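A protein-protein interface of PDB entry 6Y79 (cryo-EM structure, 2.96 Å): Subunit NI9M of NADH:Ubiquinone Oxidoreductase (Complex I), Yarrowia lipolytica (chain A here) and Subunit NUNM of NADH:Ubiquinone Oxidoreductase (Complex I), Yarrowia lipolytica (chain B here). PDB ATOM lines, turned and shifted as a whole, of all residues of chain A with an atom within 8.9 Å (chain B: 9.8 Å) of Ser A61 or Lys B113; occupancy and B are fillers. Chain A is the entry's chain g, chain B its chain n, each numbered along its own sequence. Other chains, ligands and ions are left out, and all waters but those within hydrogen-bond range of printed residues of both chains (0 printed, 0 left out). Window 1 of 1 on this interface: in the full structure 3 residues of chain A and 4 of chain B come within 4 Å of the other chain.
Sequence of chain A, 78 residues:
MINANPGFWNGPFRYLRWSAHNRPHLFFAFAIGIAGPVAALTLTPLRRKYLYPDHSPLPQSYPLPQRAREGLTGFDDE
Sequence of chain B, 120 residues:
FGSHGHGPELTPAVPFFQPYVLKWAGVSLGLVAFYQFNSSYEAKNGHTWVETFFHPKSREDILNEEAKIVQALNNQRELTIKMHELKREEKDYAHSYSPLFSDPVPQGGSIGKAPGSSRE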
ATOM      1  N   LEU A  58     -17.643 -27.516   5.412  1.00  0.00           N
ATOM      2  CA  LEU A  58     -17.843 -28.727   6.173  1.00  0.00           C
ATOM      3  C   LEU A  58     -18.940 -28.513   7.214  1.00  0.00           C
ATOM      4  O   LEU A  58     -19.045 -27.425   7.785  1.00  0.00           O
ATOM      5  CB  LEU A  58     -16.537 -29.102   6.862  1.00  0.00           C
ATOM      6  CG  LEU A  58     -15.273 -29.360   6.043  1.00  0.00           C
ATOM      7  CD1 LEU A  58     -14.223 -30.035   6.903  1.00  0.00           C
ATOM      8  CD2 LEU A  58     -15.566 -30.198   4.841  1.00  0.00           C
ATOM      9  N   PRO A  59     -19.782 -29.509   7.473  1.00  0.00           N
ATOM     10  CA  PRO A  59     -20.680 -29.415   8.623  1.00  0.00           C
ATOM     11  C   PRO A  59     -19.917 -29.548   9.933  1.00  0.00           C
ATOM     12  O   PRO A  59     -18.846 -30.148  10.008  1.00  0.00           O
ATOM     13  CB  PRO A  59     -21.654 -30.577   8.410  1.00  0.00           C
ATOM     14  CG  PRO A  59     -20.940 -31.508   7.482  1.00  0.00           C
ATOM     15  CD  PRO A  59     -20.157 -30.617   6.583  1.00  0.00           C
ATOM     16  N   GLN A  60     -20.479 -28.939  10.969  1.00  0.00           N
ATOM     17  CA  GLN A  60     -19.886 -28.902  12.296  1.00  0.00           C
ATOM     18  C   GLN A  60     -20.759 -29.523  13.369  1.00  0.00           C
ATOM     19  O   GLN A  60     -20.232 -30.038  14.354  1.00  0.00           O
ATOM     20  CB  GLN A  60     -19.581 -27.460  12.696  1.00  0.00           C
ATOM     21  CG  GLN A  60     -18.477 -26.832  11.901  1.00  0.00           C
ATOM     22  CD  GLN A  60     -18.439 -25.342  12.098  1.00  0.00           C
ATOM     23  OE1 GLN A  60     -19.349 -24.763  12.688  1.00  0.00           O
ATOM     24  NE2 GLN A  60     -17.385 -24.708  11.613  1.00  0.00           N
ATOM     25  N   SER A  61     -22.071 -29.506  13.194  1.00  0.00           N
ATOM     26  CA  SER A  61     -22.990 -30.103  14.141  1.00  0.00           C
ATOM     27  C   SER A  61     -23.851 -31.104  13.394  1.00  0.00           C
ATOM     28  O   SER A  61     -23.563 -31.417  12.238  1.00  0.00           O
ATOM     29  CB  SER A  61     -23.844 -29.021  14.785  1.00  0.00           C
ATOM     30  OG  SER A  61     -24.636 -28.381  13.799  1.00  0.00           O
ATOM     31  N   TYR A  62     -24.887 -31.626  14.022  1.00  0.00           N
ATOM     32  CA  TYR A  62     -25.940 -32.230  13.229  1.00  0.00           C
ATOM     33  C   TYR A  62     -26.673 -31.115  12.495  1.00  0.00           C
ATOM     34  O   TYR A  62     -27.029 -30.106  13.113  1.00  0.00           O
ATOM     35  CB  TYR A  62     -26.924 -33.030  14.073  1.00  0.00           C
ATOM     36  CG  TYR A  62     -27.946 -33.752  13.226  1.00  0.00           C
ATOM     37  CD1 TYR A  62     -27.642 -34.962  12.620  1.00  0.00           C
ATOM     38  CD2 TYR A  62     -29.208 -33.212  13.014  1.00  0.00           C
ATOM     39  CE1 TYR A  62     -28.569 -35.616  11.838  1.00  0.00           C
ATOM     40  CE2 TYR A  62     -30.130 -33.851  12.226  1.00  0.00           C
ATOM     41  CZ  TYR A  62     -29.810 -35.054  11.646  1.00  0.00           C
ATOM     42  OH  TYR A  62     -30.737 -35.700  10.869  1.00  0.00           O
ATOM     43  N   PRO A  63     -26.915 -31.251  11.204  1.00  0.00           N
ATOM     44  CA  PRO A  63     -27.673 -30.225  10.485  1.00  0.00           C
ATOM     45  C   PRO A  63     -29.163 -30.285  10.781  1.00  0.00           C
ATOM     46  O   PRO A  63     -29.869 -31.189  10.324  1.00  0.00           O
ATOM     47  CB  PRO A  63     -27.374 -30.540   9.015  1.00  0.00           C
ATOM     48  CG  PRO A  63     -27.032 -31.977   8.994  1.00  0.00           C
ATOM     49  CD  PRO A  63     -26.439 -32.317  10.316  1.00  0.00           C
ATOM     50  N   LEU A  64     -29.647 -29.336  11.555  1.00  0.00           N
ATOM     51  CA  LEU A  64     -31.084 -29.237  11.774  1.00  0.00           C
ATOM     52  C   LEU A  64     -31.721 -28.455  10.640  1.00  0.00           C
ATOM     53  O   LEU A  64     -31.291 -27.331  10.359  1.00  0.00           O
ATOM     54  CB  LEU A  64     -31.393 -28.532  13.083  1.00  0.00           C
ATOM     55  CG  LEU A  64     -31.073 -29.196  14.412  1.00  0.00           C
ATOM     56  CD1 LEU A  64     -31.298 -28.196  15.524  1.00  0.00           C
ATOM     57  CD2 LEU A  64     -31.954 -30.400  14.597  1.00  0.00           C
ATOM     58  N   GLN A  66     -35.457 -26.644   9.231  1.00  0.00           N
ATOM     59  CA  GLN A  66     -36.420 -25.792   9.928  1.00  0.00           C
ATOM     60  C   GLN A  66     -37.817 -26.153   9.441  1.00  0.00           C
ATOM     61  O   GLN A  66     -38.375 -25.504   8.556  1.00  0.00           O
ATOM     62  CB  GLN A  66     -36.098 -24.310   9.693  1.00  0.00           C
ATOM     63  CG  GLN A  66     -34.779 -23.846  10.296  1.00  0.00           C
ATOM     64  CD  GLN A  66     -33.588 -24.130   9.400  1.00  0.00           C
ATOM     65  OE1 GLN A  66     -33.747 -24.416   8.215  1.00  0.00           O
ATOM     66  NE2 GLN A  66     -32.389 -24.065   9.967  1.00  0.00           N
ATOM     67  N   GLN B 107     -26.916 -16.982  21.818  1.00  0.00           N
ATOM     68  CA  GLN B 107     -26.764 -18.088  20.840  1.00  0.00           C
ATOM     69  C   GLN B 107     -25.302 -18.389  20.490  1.00  0.00           C
ATOM     70  O   GLN B 107     -24.932 -18.580  19.331  1.00  0.00           O
ATOM     71  CB  GLN B 107     -27.614 -17.863  19.578  1.00  0.00           C
ATOM     72  CG  GLN B 107     -27.375 -16.606  18.801  1.00  0.00           C
ATOM     73  CD  GLN B 107     -28.058 -16.632  17.475  1.00  0.00           C
ATOM     74  OE1 GLN B 107     -29.174 -17.150  17.346  1.00  0.00           O
ATOM     75  NE2 GLN B 107     -27.353 -16.144  16.443  1.00  0.00           N
ATOM     76  N   GLY B 108     -24.464 -18.474  21.520  1.00  0.00           N
ATOM     77  CA  GLY B 108     -23.024 -18.502  21.340  1.00  0.00           C
ATOM     78  C   GLY B 108     -22.455 -19.902  21.470  1.00  0.00           C
ATOM     79  O   GLY B 108     -22.945 -20.712  22.255  1.00  0.00           O
ATOM     80  N   GLY B 109     -21.394 -20.159  20.715  1.00  0.00           N
ATOM     81  CA  GLY B 109     -20.731 -21.449  20.752  1.00  0.00           C
ATOM     82  C   GLY B 109     -21.172 -22.397  19.654  1.00  0.00           C
ATOM     83  O   GLY B 109     -21.668 -23.492  19.925  1.00  0.00           O
ATOM     84  N   SER B 110     -21.055 -21.976  18.399  1.00  0.00           N
ATOM     85  CA  SER B 110     -21.686 -22.715  17.311  1.00  0.00           C
ATOM     86  C   SER B 110     -20.708 -23.553  16.486  1.00  0.00           C
ATOM     87  O   SER B 110     -20.497 -23.282  15.305  1.00  0.00           O
ATOM     88  CB  SER B 110     -22.445 -21.745  16.427  1.00  0.00           C
ATOM     89  OG  SER B 110     -23.075 -22.429  15.364  1.00  0.00           O
ATOM     90  N   ILE B 111     -20.157 -24.631  17.087  1.00  0.00           N
ATOM     91  CA  ILE B 111     -19.625 -25.717  16.256  1.00  0.00           C
ATOM     92  C   ILE B 111     -20.162 -27.078  16.717  1.00  0.00           C
ATOM     93  O   ILE B 111     -20.785 -27.780  15.926  1.00  0.00           O
ATOM     94  CB  ILE B 111     -18.072 -25.732  16.124  1.00  0.00           C
ATOM     95  CG1 ILE B 111     -17.272 -25.907  17.418  1.00  0.00           C
ATOM     96  CG2 ILE B 111     -17.515 -24.504  15.401  1.00  0.00           C
ATOM     97  CD1 ILE B 111     -15.827 -26.159  17.135  1.00  0.00           C
ATOM     98  N   GLY B 112     -19.970 -27.477  17.971  1.00  0.00           N
ATOM     99  CA  GLY B 112     -20.282 -28.853  18.325  1.00  0.00           C
ATOM    100  C   GLY B 112     -21.623 -28.943  19.008  1.00  0.00           C
ATOM    101  O   GLY B 112     -21.804 -29.696  19.968  1.00  0.00           O
ATOM    102  N   LYS B 113     -22.575 -28.168  18.506  1.00  0.00           N
ATOM    103  CA  LYS B 113     -23.749 -27.826  19.285  1.00  0.00           C
ATOM    104  C   LYS B 113     -24.781 -28.942  19.235  1.00  0.00           C
ATOM    105  O   LYS B 113     -24.894 -29.672  18.246  1.00  0.00           O
ATOM    106  CB  LYS B 113     -24.322 -26.489  18.805  1.00  0.00           C
ATOM    107  CG  LYS B 113     -25.554 -26.541  17.944  1.00  0.00           C
ATOM    108  CD  LYS B 113     -25.915 -25.156  17.458  1.00  0.00           C
ATOM    109  CE  LYS B 113     -27.215 -25.181  16.687  1.00  0.00           C
ATOM    110  NZ  LYS B 113     -27.574 -23.842  16.159  1.00  0.00           N
ATOM    111  N   ALA B 114     -25.480 -29.098  20.327  1.00  0.00           N
ATOM    112  CA  ALA B 114     -26.508 -30.093  20.573  1.00  0.00           C
ATOM    113  C   ALA B 114     -27.864 -29.518  20.210  1.00  0.00           C
ATOM    114  O   ALA B 114     -28.122 -28.347  20.497  1.00  0.00           O
ATOM    115  CB  ALA B 114     -26.501 -30.508  22.036  1.00  0.00           C
ATOM    116  N   PRO B 115     -28.729 -30.254  19.519  1.00  0.00           N
ATOM    117  CA  PRO B 115     -30.133 -29.834  19.458  1.00  0.00           C
ATOM    118  C   PRO B 115     -30.843 -30.094  20.779  1.00  0.00           C
ATOM    119  O   PRO B 115     -30.649 -31.129  21.417  1.00  0.00           O
ATOM    120  CB  PRO B 115     -30.703 -30.672  18.312  1.00  0.00           C
ATOM    121  CG  PRO B 115     -29.516 -30.869  17.426  1.00  0.00           C
ATOM    122  CD  PRO B 115     -28.388 -31.124  18.381  1.00  0.00           C
ATOM    123  N   GLY B 116     -31.664 -29.131  21.191  1.00  0.00           N
ATOM    124  CA  GLY B 116     -32.204 -29.101  22.528  1.00  0.00           C
ATOM    125  C   GLY B 116     -31.463 -28.191  23.478  1.00  0.00           C
ATOM    126  O   GLY B 116     -31.723 -28.236  24.692  1.00  0.00           O
ATOM    127  N   SER B 117     -30.554 -27.364  22.965  1.00  0.00           N
ATOM    128  CA  SER B 117     -29.678 -26.560  23.796  1.00  0.00           C
ATOM    129  C   SER B 117     -30.168 -25.130  23.948  1.00  0.00           C
ATOM    130  O   SER B 117     -29.466 -24.300  24.532  1.00  0.00           O
ATOM    131  CB  SER B 117     -28.274 -26.571  23.219  1.00  0.00           C
ATOM    132  OG  SER B 117     -28.302 -25.967  21.933  1.00  0.00           O
ATOM    133  N   SER B 118     -31.360 -24.822  23.454  1.00  0.00           N
ATOM    134  CA  SER B 118     -31.731 -23.423  23.243  1.00  0.00           C
ATOM    135  C   SER B 118     -32.443 -22.823  24.454  1.00  0.00           C
ATOM    136  O   SER B 118     -31.886 -21.951  25.128  1.00  0.00           O
ATOM    137  CB  SER B 118     -32.574 -23.314  21.973  1.00  0.00           C
ATOM    138  OG  SER B 118     -31.747 -23.447  20.833  1.00  0.00           O
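The side-chain amide oxygen (OE1) of Gln A60 sits close to the backbone carbonyl oxygen (O) of Ser B110 (3.2 Å).
O of Gln A60 lies close to O of Ile B111.
The backbone NH (N) of Ser A61 lies within hydrogen-bond range of the backbone carbonyl oxygen (O) of Ile B111, at 3.5 Å.
Ser A61 touches Lys B113 (CB to O, 3.7 Å).
Leu A64 touches Pro B115 (CD1 to CG, 3.7 Å).
The backbone carbonyl oxygen (O) of Leu A64 lies within hydrogen-bond range of the side-chain amide nitrogen (NE2) of Gln A66.
Of the 8 printed residues of chain A, 3 touch a printed residue of chain B.
Printed residues of chain A that touch a printed residue of chain B: Gln A60, Ser A61 and Leu A64.
Along chain B the printed residues that touch a printed residue of chain A span positions 110 to 115.
Among the printed residues, 5 pairs touch across the chains.
Printed residues of chain B within 4 Å of Ser A61: Ile B111 and Lys B113.
No residue of chain A comes within 4 Å of Ala B114.
Printed residues of chain A within 4 Å of Pro B115: Leu A64 (3.7 Å).
Of the printed residues of chain B, Leu A64 touches Pro B115 (3.7 Å).
Of the printed residues of chain A, Ser B110 touches Gln A60.
Of the printed residues of chain B, Gln A60 touches Ser B110 and Ile B111.
Printed residues of chain A within 4 Å of Ile B111: Gln A60 and Ser A61.
Gly B108 touches none of the printed residues of chain A.
Ser B117 touches none of the printed residues of chain A.
The nearest residue of chain B that does not touch Ser A61 is Gly B112 (4.8 Å).
The nearest residue of chain A that does not touch Lys B113 is Tyr A62 (4.7 Å).
The nearest printed residue of chain A that does not touch Ser B110 is Ser A61 (6.3 Å).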
